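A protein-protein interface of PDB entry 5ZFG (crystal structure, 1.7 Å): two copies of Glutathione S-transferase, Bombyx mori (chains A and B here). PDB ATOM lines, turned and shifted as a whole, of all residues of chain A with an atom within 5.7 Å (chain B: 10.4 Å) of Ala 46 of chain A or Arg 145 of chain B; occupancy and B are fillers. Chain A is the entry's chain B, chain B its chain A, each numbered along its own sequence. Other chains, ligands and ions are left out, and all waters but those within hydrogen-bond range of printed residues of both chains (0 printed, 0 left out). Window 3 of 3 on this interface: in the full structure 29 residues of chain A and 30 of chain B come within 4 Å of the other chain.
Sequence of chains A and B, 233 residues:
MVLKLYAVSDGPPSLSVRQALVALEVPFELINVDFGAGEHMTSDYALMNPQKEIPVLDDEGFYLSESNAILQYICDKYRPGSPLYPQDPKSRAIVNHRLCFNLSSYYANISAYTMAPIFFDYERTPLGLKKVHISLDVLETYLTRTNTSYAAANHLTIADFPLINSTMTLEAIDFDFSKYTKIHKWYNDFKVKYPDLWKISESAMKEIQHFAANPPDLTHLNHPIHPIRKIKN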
ATOM      1  N   HIS A  40     -17.815  31.068  29.170  1.00  0.00           N
ATOM      2  CA  HIS A  40     -17.479  30.585  27.833  1.00  0.00           C
ATOM      3  C   HIS A  40     -16.201  29.755  27.795  1.00  0.00           C
ATOM      4  O   HIS A  40     -15.882  29.189  26.741  1.00  0.00           O
ATOM      5  CB  HIS A  40     -17.353  31.764  26.873  1.00  0.00           C
ATOM      6  CG  HIS A  40     -16.304  32.753  27.280  1.00  0.00           C
ATOM      7  ND1 HIS A  40     -16.338  33.419  28.487  1.00  0.00           N
ATOM      8  CD2 HIS A  40     -15.191  33.185  26.643  1.00  0.00           C
ATOM      9  CE1 HIS A  40     -15.285  34.214  28.577  1.00  0.00           C
ATOM     10  NE2 HIS A  40     -14.577  34.094  27.468  1.00  0.00           N
ATOM     11  N   THR A  42     -15.551  27.127  29.990  1.00  0.00           N
ATOM     12  CA  THR A  42     -15.716  25.825  30.627  1.00  0.00           C
ATOM     13  C   THR A  42     -15.840  24.697  29.602  1.00  0.00           C
ATOM     14  O   THR A  42     -16.129  24.914  28.422  1.00  0.00           O
ATOM     15  CB  THR A  42     -16.950  25.830  31.523  1.00  0.00           C
ATOM     16  OG1 THR A  42     -18.107  26.064  30.707  1.00  0.00           O
ATOM     17  CG2 THR A  42     -16.826  26.926  32.592  1.00  0.00           C
ATOM     18  N   SER A  43     -15.634  23.464  30.078  1.00  0.00           N
ATOM     19  CA  SER A  43     -15.760  22.313  29.186  1.00  0.00           C
ATOM     20  C   SER A  43     -17.197  22.113  28.720  1.00  0.00           C
ATOM     21  O   SER A  43     -17.418  21.673  27.585  1.00  0.00           O
ATOM     22  CB  SER A  43     -15.240  21.042  29.862  1.00  0.00           C
ATOM     23  OG  SER A  43     -16.135  20.591  30.861  1.00  0.00           O
ATOM     24  N   ASP A  44     -18.188  22.422  29.569  1.00  0.00           N
ATOM     25  CA  ASP A  44     -19.576  22.322  29.127  1.00  0.00           C
ATOM     26  C   ASP A  44     -19.841  23.256  27.952  1.00  0.00           C
ATOM     27  O   ASP A  44     -20.499  22.869  26.979  1.00  0.00           O
ATOM     28  CB  ASP A  44     -20.534  22.636  30.277  1.00  0.00           C
ATOM     29  CG  ASP A  44     -20.963  21.393  31.051  1.00  0.00           C
ATOM     30  OD1 ASP A  44     -20.674  20.262  30.602  1.00  0.00           O
ATOM     31  OD2 ASP A  44     -21.598  21.553  32.118  1.00  0.00           O
ATOM     32  N   TYR A  45     -19.335  24.491  28.024  1.00  0.00           N
ATOM     33  CA  TYR A  45     -19.499  25.406  26.895  1.00  0.00           C
ATOM     34  C   TYR A  45     -18.745  24.899  25.676  1.00  0.00           C
ATOM     35  O   TYR A  45     -19.244  24.994  24.547  1.00  0.00           O
ATOM     36  CB  TYR A  45     -19.032  26.813  27.263  1.00  0.00           C
ATOM     37  CG  TYR A  45     -19.418  27.860  26.229  1.00  0.00           C
ATOM     38  CD1 TYR A  45     -20.621  28.545  26.316  1.00  0.00           C
ATOM     39  CD2 TYR A  45     -18.567  28.161  25.166  1.00  0.00           C
ATOM     40  CE1 TYR A  45     -20.979  29.500  25.368  1.00  0.00           C
ATOM     41  CE2 TYR A  45     -18.911  29.117  24.221  1.00  0.00           C
ATOM     42  CZ  TYR A  45     -20.118  29.779  24.322  1.00  0.00           C
ATOM     43  OH  TYR A  45     -20.454  30.738  23.389  1.00  0.00           O
ATOM     44  N   ALA A  46     -17.548  24.341  25.884  1.00  0.00           N
ATOM     45  CA  ALA A  46     -16.782  23.806  24.767  1.00  0.00           C
ATOM     46  C   ALA A  46     -17.452  22.593  24.120  1.00  0.00           C
ATOM     47  O   ALA A  46     -17.181  22.312  22.948  1.00  0.00           O
ATOM     48  CB  ALA A  46     -15.363  23.453  25.226  1.00  0.00           C
ATOM     49  N   LEU A  47     -18.321  21.870  24.842  1.00  0.00           N
ATOM     50  CA  LEU A  47     -19.139  20.848  24.188  1.00  0.00           C
ATOM     51  C   LEU A  47     -19.948  21.436  23.042  1.00  0.00           C
ATOM     52  O   LEU A  47     -20.197  20.757  22.038  1.00  0.00           O
ATOM     53  CB  LEU A  47     -20.099  20.201  25.186  1.00  0.00           C
ATOM     54  CG  LEU A  47     -19.611  19.054  26.063  1.00  0.00           C
ATOM     55  CD1 LEU A  47     -20.727  18.674  27.027  1.00  0.00           C
ATOM     56  CD2 LEU A  47     -19.205  17.863  25.202  1.00  0.00           C
ATOM     57  N   MET A  48     -20.381  22.684  23.183  1.00  0.00           N
ATOM     58  CA  MET A  48     -21.139  23.358  22.139  1.00  0.00           C
ATOM     59  C   MET A  48     -20.233  24.057  21.136  1.00  0.00           C
ATOM     60  O   MET A  48     -20.466  23.969  19.923  1.00  0.00           O
ATOM     61  CB  MET A  48     -22.103  24.364  22.763  1.00  0.00           C
ATOM     62  CG  MET A  48     -23.200  23.747  23.620  1.00  0.00           C
ATOM     63  SD  MET A  48     -24.414  24.982  24.141  1.00  0.00           S
ATOM     64  CE  MET A  48     -23.400  26.027  25.199  1.00  0.00           C
ATOM     65  N   ASN A  49     -19.203  24.754  21.621  1.00  0.00           N
ATOM     66  CA  ASN A  49     -18.294  25.511  20.765  1.00  0.00           C
ATOM     67  C   ASN A  49     -16.860  25.266  21.214  1.00  0.00           C
ATOM     68  O   ASN A  49     -16.353  25.962  22.107  1.00  0.00           O
ATOM     69  CB  ASN A  49     -18.599  27.005  20.787  1.00  0.00           C
ATOM     70  CG  ASN A  49     -17.723  27.754  19.813  1.00  0.00           C
ATOM     71  OD1 ASN A  49     -17.074  27.123  18.983  1.00  0.00           O
ATOM     72  ND2 ASN A  49     -17.708  29.080  19.886  1.00  0.00           N
ATOM     73  N   PRO A  50     -16.159  24.315  20.594  1.00  0.00           N
ATOM     74  CA  PRO A  50     -14.753  24.074  20.967  1.00  0.00           C
ATOM     75  C   PRO A  50     -13.851  25.282  20.766  1.00  0.00           C
ATOM     76  O   PRO A  50     -12.740  25.308  21.314  1.00  0.00           O
ATOM     77  CB  PRO A  50     -14.342  22.907  20.058  1.00  0.00           C
ATOM     78  CG  PRO A  50     -15.277  22.972  18.905  1.00  0.00           C
ATOM     79  CD  PRO A  50     -16.595  23.463  19.475  1.00  0.00           C
ATOM     80  N   LYS A  52     -14.566  28.213  22.005  1.00  0.00           N
ATOM     81  CA  LYS A  52     -14.667  28.985  23.249  1.00  0.00           C
ATOM     82  C   LYS A  52     -14.999  30.449  22.991  1.00  0.00           C
ATOM     83  O   LYS A  52     -14.525  31.340  23.703  1.00  0.00           O
ATOM     84  CB  LYS A  52     -13.378  28.902  24.072  1.00  0.00           C
ATOM     85  CG  LYS A  52     -12.813  27.517  24.264  1.00  0.00           C
ATOM     86  CD  LYS A  52     -11.690  27.586  25.321  1.00  0.00           C
ATOM     87  CE  LYS A  52     -11.382  26.232  25.921  1.00  0.00           C
ATOM     88  NZ  LYS A  52     -12.557  25.630  26.606  1.00  0.00           N
ATOM     89  N   LYS B  90     -28.763  22.342   7.191  1.00  0.00           N
ATOM     90  CA  LYS B  90     -27.834  21.889   8.221  1.00  0.00           C
ATOM     91  C   LYS B  90     -26.482  21.507   7.630  1.00  0.00           C
ATOM     92  O   LYS B  90     -25.429  21.914   8.140  1.00  0.00           O
ATOM     93  CB  LYS B  90     -28.435  20.708   8.982  1.00  0.00           C
ATOM     94  CG  LYS B  90     -27.531  20.158  10.072  1.00  0.00           C
ATOM     95  CD  LYS B  90     -28.313  19.214  10.969  1.00  0.00           C
ATOM     96  CE  LYS B  90     -27.403  18.437  11.893  1.00  0.00           C
ATOM     97  NZ  LYS B  90     -28.221  17.559  12.795  1.00  0.00           N
ATOM     98  N   ILE B  94     -22.655  23.398   8.208  1.00  0.00           N
ATOM     99  CA  ILE B  94     -21.363  22.841   8.606  1.00  0.00           C
ATOM    100  C   ILE B  94     -20.267  23.324   7.660  1.00  0.00           C
ATOM    101  O   ILE B  94     -19.171  23.695   8.099  1.00  0.00           O
ATOM    102  CB  ILE B  94     -21.410  21.302   8.684  1.00  0.00           C
ATOM    103  CG1 ILE B  94     -22.509  20.855   9.659  1.00  0.00           C
ATOM    104  CG2 ILE B  94     -20.035  20.761   9.163  1.00  0.00           C
ATOM    105  CD1 ILE B  94     -22.820  19.360   9.606  1.00  0.00           C
ATOM    106  N   HIS B  97     -19.688  27.023   8.440  1.00  0.00           N
ATOM    107  CA  HIS B  97     -18.931  27.152   9.676  1.00  0.00           C
ATOM    108  C   HIS B  97     -17.445  26.913   9.437  1.00  0.00           C
ATOM    109  O   HIS B  97     -16.588  27.693   9.881  1.00  0.00           O
ATOM    110  CB  HIS B  97     -19.422  26.169  10.736  1.00  0.00           C
ATOM    111  CG  HIS B  97     -18.510  26.154  11.916  1.00  0.00           C
ATOM    112  ND1 HIS B  97     -17.398  25.342  11.977  1.00  0.00           N
ATOM    113  CD2 HIS B  97     -18.439  26.974  12.992  1.00  0.00           C
ATOM    114  CE1 HIS B  97     -16.717  25.617  13.076  1.00  0.00           C
ATOM    115  NE2 HIS B  97     -17.327  26.604  13.708  1.00  0.00           N
ATOM    116  N   ARG B  98     -17.120  25.812   8.747  1.00  0.00           N
ATOM    117  CA  ARG B  98     -15.718  25.470   8.544  1.00  0.00           C
ATOM    118  C   ARG B  98     -14.987  26.536   7.732  1.00  0.00           C
ATOM    119  O   ARG B  98     -13.800  26.794   7.978  1.00  0.00           O
ATOM    120  CB  ARG B  98     -15.604  24.090   7.874  1.00  0.00           C
ATOM    121  CG  ARG B  98     -16.161  22.899   8.704  1.00  0.00           C
ATOM    122  CD  ARG B  98     -15.454  22.684  10.040  1.00  0.00           C
ATOM    123  NE  ARG B  98     -15.951  21.455  10.674  1.00  0.00           N
ATOM    124  CZ  ARG B  98     -17.005  21.384  11.485  1.00  0.00           C
ATOM    125  NH1 ARG B  98     -17.695  22.474  11.811  1.00  0.00           N
ATOM    126  NH2 ARG B  98     -17.372  20.207  11.971  1.00  0.00           N
ATOM    127  N   ILE B 134      -3.520  24.851  19.452  1.00  0.00           N
ATOM    128  CA  ILE B 134      -4.928  25.003  19.807  1.00  0.00           C
ATOM    129  C   ILE B 134      -5.811  24.901  18.564  1.00  0.00           C
ATOM    130  O   ILE B 134      -6.864  24.247  18.584  1.00  0.00           O
ATOM    131  CB  ILE B 134      -5.134  26.327  20.568  1.00  0.00           C
ATOM    132  CG1 ILE B 134      -4.510  26.220  21.965  1.00  0.00           C
ATOM    133  CG2 ILE B 134      -6.608  26.666  20.678  1.00  0.00           C
ATOM    134  CD1 ILE B 134      -4.010  27.520  22.518  1.00  0.00           C
ATOM    135  N   ASP B 137      -5.954  21.403  17.602  1.00  0.00           N
ATOM    136  CA  ASP B 137      -6.774  20.657  18.548  1.00  0.00           C
ATOM    137  C   ASP B 137      -8.260  20.885  18.287  1.00  0.00           C
ATOM    138  O   ASP B 137      -9.065  19.947  18.386  1.00  0.00           O
ATOM    139  CB  ASP B 137      -6.397  21.032  19.981  1.00  0.00           C
ATOM    140  CG  ASP B 137      -6.993  20.082  20.999  1.00  0.00           C
ATOM    141  OD1 ASP B 137      -6.641  18.883  20.974  1.00  0.00           O
ATOM    142  OD2 ASP B 137      -7.828  20.534  21.807  1.00  0.00           O
ATOM    143  N   VAL B 138      -8.636  22.109  17.913  1.00  0.00           N
ATOM    144  CA  VAL B 138     -10.035  22.400  17.611  1.00  0.00           C
ATOM    145  C   VAL B 138     -10.480  21.654  16.353  1.00  0.00           C
ATOM    146  O   VAL B 138     -11.529  20.996  16.346  1.00  0.00           O
ATOM    147  CB  VAL B 138     -10.261  23.923  17.499  1.00  0.00           C
ATOM    148  CG1 VAL B 138     -11.629  24.234  16.879  1.00  0.00           C
ATOM    149  CG2 VAL B 138     -10.146  24.585  18.862  1.00  0.00           C
ATOM    150  N   LEU B 139      -9.682  21.703  15.280  1.00  0.00           N
ATOM    151  CA  LEU B 139     -10.076  20.973  14.074  1.00  0.00           C
ATOM    152  C   LEU B 139     -10.098  19.471  14.328  1.00  0.00           C
ATOM    153  O   LEU B 139     -11.001  18.765  13.858  1.00  0.00           O
ATOM    154  CB  LEU B 139      -9.151  21.315  12.899  1.00  0.00           C
ATOM    155  CG  LEU B 139      -9.477  20.585  11.586  1.00  0.00           C
ATOM    156  CD1 LEU B 139     -10.908  20.849  11.094  1.00  0.00           C
ATOM    157  CD2 LEU B 139      -8.449  20.915  10.501  1.00  0.00           C
ATOM    158  N   GLU B 140      -9.129  18.968  15.101  1.00  0.00           N
ATOM    159  CA  GLU B 140      -9.160  17.567  15.509  1.00  0.00           C
ATOM    160  C   GLU B 140     -10.445  17.259  16.270  1.00  0.00           C
ATOM    161  O   GLU B 140     -11.069  16.209  16.060  1.00  0.00           O
ATOM    162  CB  GLU B 140      -7.918  17.243  16.353  1.00  0.00           C
ATOM    163  CG  GLU B 140      -7.790  15.759  16.771  1.00  0.00           C
ATOM    164  CD  GLU B 140      -7.242  14.860  15.671  1.00  0.00           C
ATOM    165  OE1 GLU B 140      -6.787  15.383  14.632  1.00  0.00           O
ATOM    166  OE2 GLU B 140      -7.264  13.619  15.842  1.00  0.00           O
ATOM    167  N   THR B 141     -10.872  18.183  17.134  1.00  0.00           N
ATOM    168  CA  THR B 141     -12.108  17.994  17.884  1.00  0.00           C
ATOM    169  C   THR B 141     -13.307  17.930  16.948  1.00  0.00           C
ATOM    170  O   THR B 141     -14.172  17.055  17.088  1.00  0.00           O
ATOM    171  CB  THR B 141     -12.276  19.115  18.913  1.00  0.00           C
ATOM    172  OG1 THR B 141     -11.231  19.029  19.888  1.00  0.00           O
ATOM    173  CG2 THR B 141     -13.622  19.006  19.612  1.00  0.00           C
ATOM    174  N   TYR B 142     -13.372  18.854  15.979  1.00  0.00           N
ATOM    175  CA  TYR B 142     -14.493  18.856  15.046  1.00  0.00           C
ATOM    176  C   TYR B 142     -14.550  17.551  14.257  1.00  0.00           C
ATOM    177  O   TYR B 142     -15.623  16.955  14.110  1.00  0.00           O
ATOM    178  CB  TYR B 142     -14.399  20.067  14.108  1.00  0.00           C
ATOM    179  CG  TYR B 142     -14.959  21.363  14.689  1.00  0.00           C
ATOM    180  CD1 TYR B 142     -16.255  21.424  15.210  1.00  0.00           C
ATOM    181  CD2 TYR B 142     -14.183  22.524  14.724  1.00  0.00           C
ATOM    182  CE1 TYR B 142     -16.765  22.622  15.740  1.00  0.00           C
ATOM    183  CE2 TYR B 142     -14.676  23.713  15.262  1.00  0.00           C
ATOM    184  CZ  TYR B 142     -15.976  23.757  15.756  1.00  0.00           C
ATOM    185  OH  TYR B 142     -16.480  24.934  16.288  1.00  0.00           O
ATOM    186  N   LEU B 143     -13.397  17.068  13.780  1.00  0.00           N
ATOM    187  CA  LEU B 143     -13.375  15.822  13.014  1.00  0.00           C
ATOM    188  C   LEU B 143     -13.805  14.634  13.868  1.00  0.00           C
ATOM    189  O   LEU B 143     -14.477  13.719  13.375  1.00  0.00           O
ATOM    190  CB  LEU B 143     -11.976  15.580  12.439  1.00  0.00           C
ATOM    191  CG  LEU B 143     -11.509  16.523  11.328  1.00  0.00           C
ATOM    192  CD1 LEU B 143     -10.016  16.324  11.071  1.00  0.00           C
ATOM    193  CD2 LEU B 143     -12.328  16.310  10.049  1.00  0.00           C
ATOM    194  N   THR B 144     -13.426  14.637  15.150  1.00  0.00           N
ATOM    195  CA  THR B 144     -13.833  13.573  16.069  1.00  0.00           C
ATOM    196  C   THR B 144     -15.341  13.578  16.274  1.00  0.00           C
ATOM    197  O   THR B 144     -15.980  12.520  16.261  1.00  0.00           O
ATOM    198  CB  THR B 144     -13.115  13.724  17.417  1.00  0.00           C
ATOM    199  OG1 THR B 144     -11.700  13.812  17.219  1.00  0.00           O
ATOM    200  CG2 THR B 144     -13.416  12.531  18.337  1.00  0.00           C
ATOM    201  N   ARG B 145     -15.930  14.760  16.459  1.00  0.00           N
ATOM    202  CA  ARG B 145     -17.352  14.827  16.772  1.00  0.00           C
ATOM    203  C   ARG B 145     -18.212  14.499  15.559  1.00  0.00           C
ATOM    204  O   ARG B 145     -19.224  13.798  15.684  1.00  0.00           O
ATOM    205  CB  ARG B 145     -17.699  16.207  17.336  1.00  0.00           C
ATOM    206  CG  ARG B 145     -16.982  16.489  18.647  1.00  0.00           C
ATOM    207  CD  ARG B 145     -17.439  17.786  19.295  1.00  0.00           C
ATOM    208  NE  ARG B 145     -16.672  18.107  20.503  1.00  0.00           N
ATOM    209  CZ  ARG B 145     -16.790  19.258  21.157  1.00  0.00           C
ATOM    210  NH1 ARG B 145     -17.636  20.178  20.711  1.00  0.00           N
ATOM    211  NH2 ARG B 145     -16.071  19.494  22.247  1.00  0.00           N
ATOM    212  N   THR B 146     -17.841  14.995  14.378  1.00  0.00           N
ATOM    213  CA  THR B 146     -18.591  14.617  13.191  1.00  0.00           C
ATOM    214  C   THR B 146     -18.289  13.191  12.762  1.00  0.00           C
ATOM    215  O   THR B 146     -19.124  12.575  12.089  1.00  0.00           O
ATOM    216  CB  THR B 146     -18.303  15.563  12.016  1.00  0.00           C
ATOM    217  OG1 THR B 146     -16.906  15.529  11.699  1.00  0.00           O
ATOM    218  CG2 THR B 146     -18.730  17.006  12.343  1.00  0.00           C
ATOM    219  N   ASN B 147     -17.124  12.659  13.141  1.00  0.00           N
ATOM    220  CA  ASN B 147     -16.694  11.322  12.726  1.00  0.00           C
ATOM    221  C   ASN B 147     -16.786  11.169  11.207  1.00  0.00           C
ATOM    222  O   ASN B 147     -17.245  10.151  10.686  1.00  0.00           O
ATOM    223  CB  ASN B 147     -17.511  10.243  13.442  1.00  0.00           C
ATOM    224  CG  ASN B 147     -16.850   8.886  13.403  1.00  0.00           C
ATOM    225  OD1 ASN B 147     -15.631   8.766  13.535  1.00  0.00           O
ATOM    226  ND2 ASN B 147     -17.657   7.846  13.228  1.00  0.00           N
ATOM    227  N   THR B 148     -16.363  12.210  10.489  1.00  0.00           N
ATOM    228  CA  THR B 148     -16.424  12.246   9.036  1.00  0.00           C
ATOM    229  C   THR B 148     -15.021  12.165   8.450  1.00  0.00           C
ATOM    230  O   THR B 148     -14.030  12.535   9.092  1.00  0.00           O
ATOM    231  CB  THR B 148     -17.102  13.526   8.527  1.00  0.00           C
ATOM    232  OG1 THR B 148     -16.488  14.658   9.151  1.00  0.00           O
ATOM    233  CG2 THR B 148     -18.599  13.526   8.839  1.00  0.00           C
ATOM    234  N   SER B 149     -14.955  11.688   7.202  1.00  0.00           N
ATOM    235  CA  SER B 149     -13.663  11.578   6.535  1.00  0.00           C
ATOM    236  C   SER B 149     -13.151  12.938   6.075  1.00  0.00           C
ATOM    237  O   SER B 149     -11.938  13.119   5.920  1.00  0.00           O
ATOM    238  CB  SER B 149     -13.760  10.624   5.346  1.00  0.00           C
ATOM    239  OG  SER B 149     -14.923  10.874   4.574  1.00  0.00           O
ATOM    240  N   TYR B 150     -14.049  13.890   5.839  1.00  0.00           N
ATOM    241  CA  TYR B 150     -13.684  15.228   5.386  1.00  0.00           C
ATOM    242  C   TYR B 150     -14.166  16.264   6.404  1.00  0.00           C
ATOM    243  O   TYR B 150     -14.816  15.935   7.406  1.00  0.00           O
ATOM    244  CB  TYR B 150     -14.258  15.504   3.995  1.00  0.00           C
ATOM    245  CG  TYR B 150     -13.699  14.612   2.907  1.00  0.00           C
ATOM    246  CD1 TYR B 150     -12.567  14.981   2.192  1.00  0.00           C
ATOM    247  CD2 TYR B 150     -14.309  13.402   2.591  1.00  0.00           C
ATOM    248  CE1 TYR B 150     -12.056  14.165   1.183  1.00  0.00           C
ATOM    249  CE2 TYR B 150     -13.809  12.580   1.586  1.00  0.00           C
ATOM    250  CZ  TYR B 150     -12.685  12.967   0.888  1.00  0.00           C
ATOM    251  OH  TYR B 150     -12.186  12.153  -0.110  1.00  0.00           O
ATOM    252  N   ALA B 151     -13.853  17.537   6.129  1.00  0.00           N
ATOM    253  CA  ALA B 151     -14.011  18.564   7.161  1.00  0.00           C
ATOM    254  C   ALA B 151     -15.470  18.845   7.497  1.00  0.00           C
ATOM    255  O   ALA B 151     -15.771  19.233   8.632  1.00  0.00           O
ATOM    256  CB  ALA B 151     -13.318  19.851   6.726  1.00  0.00           C
ATOM    257  N   ALA B 152     -16.380  18.691   6.545  1.00  0.00           N
ATOM    258  CA  ALA B 152     -17.784  19.008   6.790  1.00  0.00           C
ATOM    259  C   ALA B 152     -18.744  17.876   6.454  1.00  0.00           C
ATOM    260  O   ALA B 152     -19.958  18.042   6.637  1.00  0.00           O
ATOM    261  CB  ALA B 152     -18.198  20.255   5.994  1.00  0.00           C
ATOM    262  N   ALA B 153     -18.252  16.758   5.946  1.00  0.00           N
ATOM    263  CA  ALA B 153     -19.116  15.690   5.459  1.00  0.00           C
ATOM    264  C   ALA B 153     -18.234  14.480   5.199  1.00  0.00           C
ATOM    265  O   ALA B 153     -17.010  14.543   5.339  1.00  0.00           O
ATOM    266  CB  ALA B 153     -19.878  16.110   4.200  1.00  0.00           C
ATOM    267  N   ASN B 154     -18.874  13.362   4.836  1.00  0.00           N
ATOM    268  CA  ASN B 154     -18.146  12.178   4.404  1.00  0.00           C
ATOM    269  C   ASN B 154     -17.754  12.246   2.941  1.00  0.00           C
ATOM    270  O   ASN B 154     -17.356  11.227   2.369  1.00  0.00           O
ATOM    271  CB  ASN B 154     -18.977  10.922   4.670  1.00  0.00           C
ATOM    272  CG  ASN B 154     -18.747  10.371   6.052  1.00  0.00           C
ATOM    273  OD1 ASN B 154     -17.627  10.423   6.578  1.00  0.00           O
ATOM    274  ND2 ASN B 154     -19.807   9.851   6.663  1.00  0.00           N
ATOM    275  N   LYS B 182      -6.626  12.436  13.294  1.00  0.00           N
ATOM    276  CA  LYS B 182      -7.637  12.589  12.259  1.00  0.00           C
ATOM    277  C   LYS B 182      -7.239  13.654  11.245  1.00  0.00           C
ATOM    278  O   LYS B 182      -7.485  13.487  10.048  1.00  0.00           O
ATOM    279  CB  LYS B 182      -8.991  12.901  12.897  1.00  0.00           C
ATOM    280  CG  LYS B 182      -9.413  11.832  13.911  1.00  0.00           C
ATOM    281  CD  LYS B 182     -10.729  12.164  14.582  1.00  0.00           C
ATOM    282  CE  LYS B 182     -11.180  11.032  15.501  1.00  0.00           C
ATOM    283  NZ  LYS B 182     -11.535   9.790  14.756  1.00  0.00           N
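Printed residues of chain A that touch a printed residue of chain B: Ala 46, Leu 47, Asn 49 and Pro 50. Hydrophobic or aromatic side chains of chain A that line the printed part of chain B: Pro 50. Along chain A the printed residues that touch a printed residue of chain B span positions 46 to 50. Printed residues of chain B that touch a printed residue of chain A: Val 138, Thr 141, Tyr 142 and Arg 145. Hydrophobic or aromatic side chains of chain B that line the printed part of chain A: Val 138 and Tyr 142. Along chain B the printed residues that touch a printed residue of chain A span positions 138 to 145. Among the printed residues, 7 pairs touch across the chains. Among the printed residues, no Asp or Glu carboxylate lies within 4 Å of a Lys or Arg side-chain nitrogen of the other chain.
O of Asp 137 of chain B lies within hydrogen-bond range of OG1 of Thr 141 of chain B, at 2.8 Å. The backbone carbonyl oxygen (O) of Tyr 142 of chain B is in hydrogen-bond range of the side-chain hydroxyl (OG1) of Thr 146 of chain B (3.1 Å). The side-chain hydroxyl (OH) of Tyr 142 of chain B sits at hydrogen-bond distance from a ring nitrogen (NE2) of His 97 of chain B, at 3.2 Å.
The guanidinium group (NH1) of Arg 145 of chain B sits at hydrogen-bond distance from the backbone carbonyl oxygen (O) of Leu 47 of chain A (2.9 Å). NH2 of Arg 145 of chain B sits at hydrogen-bond distance from O of Ala 46 of chain A (3.1 Å).
Asn 49 of chain A touches Tyr 142 of chain B. Pro 50 of chain A touches Val 138 of chain B (O to CG2, 3.6 Å). CB of Pro 50 of chain A touches CG2 of Thr 141 of chain B, at 3.99 Å. Pro 50 of chain A touches Tyr 142 of chain B (CG to CZ, 3.3 Å). CD of Pro 50 of chain A touches NH1 of Arg 145 of chain B (3.7 Å).
No position is printed for both chains. Of the 7 pairs that touch across the chains among the printed residues, none has its exchanged pair printed and touching as well.
Of chain B, only Arg 145 comes within 4 Å of Ala 46 of chain A. Of chain B, only Arg 145 comes within 4 Å of Leu 47 of chain A. Printed residues of chain B within 4 Å of Asn 49 of chain A: Tyr 142 (3.5 Å). Of the printed residues of chain B, Pro 50 of chain A touches Val 138 (3.6 Å), Thr 141 (3.99 Å), Tyr 142 (3.3 Å) and Arg 145 (3.7 Å). Of the printed residues of chain A, Tyr 142 of chain B touches Asn 49 and Pro 50. Of chain A, only Ala 46, Leu 47 and Pro 50 come within 4 Å of Arg 145 of chain B. The nearest printed residue of chain B that does not touch Pro 50 of chain A is Asp 137 of chain B (6.3 Å).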
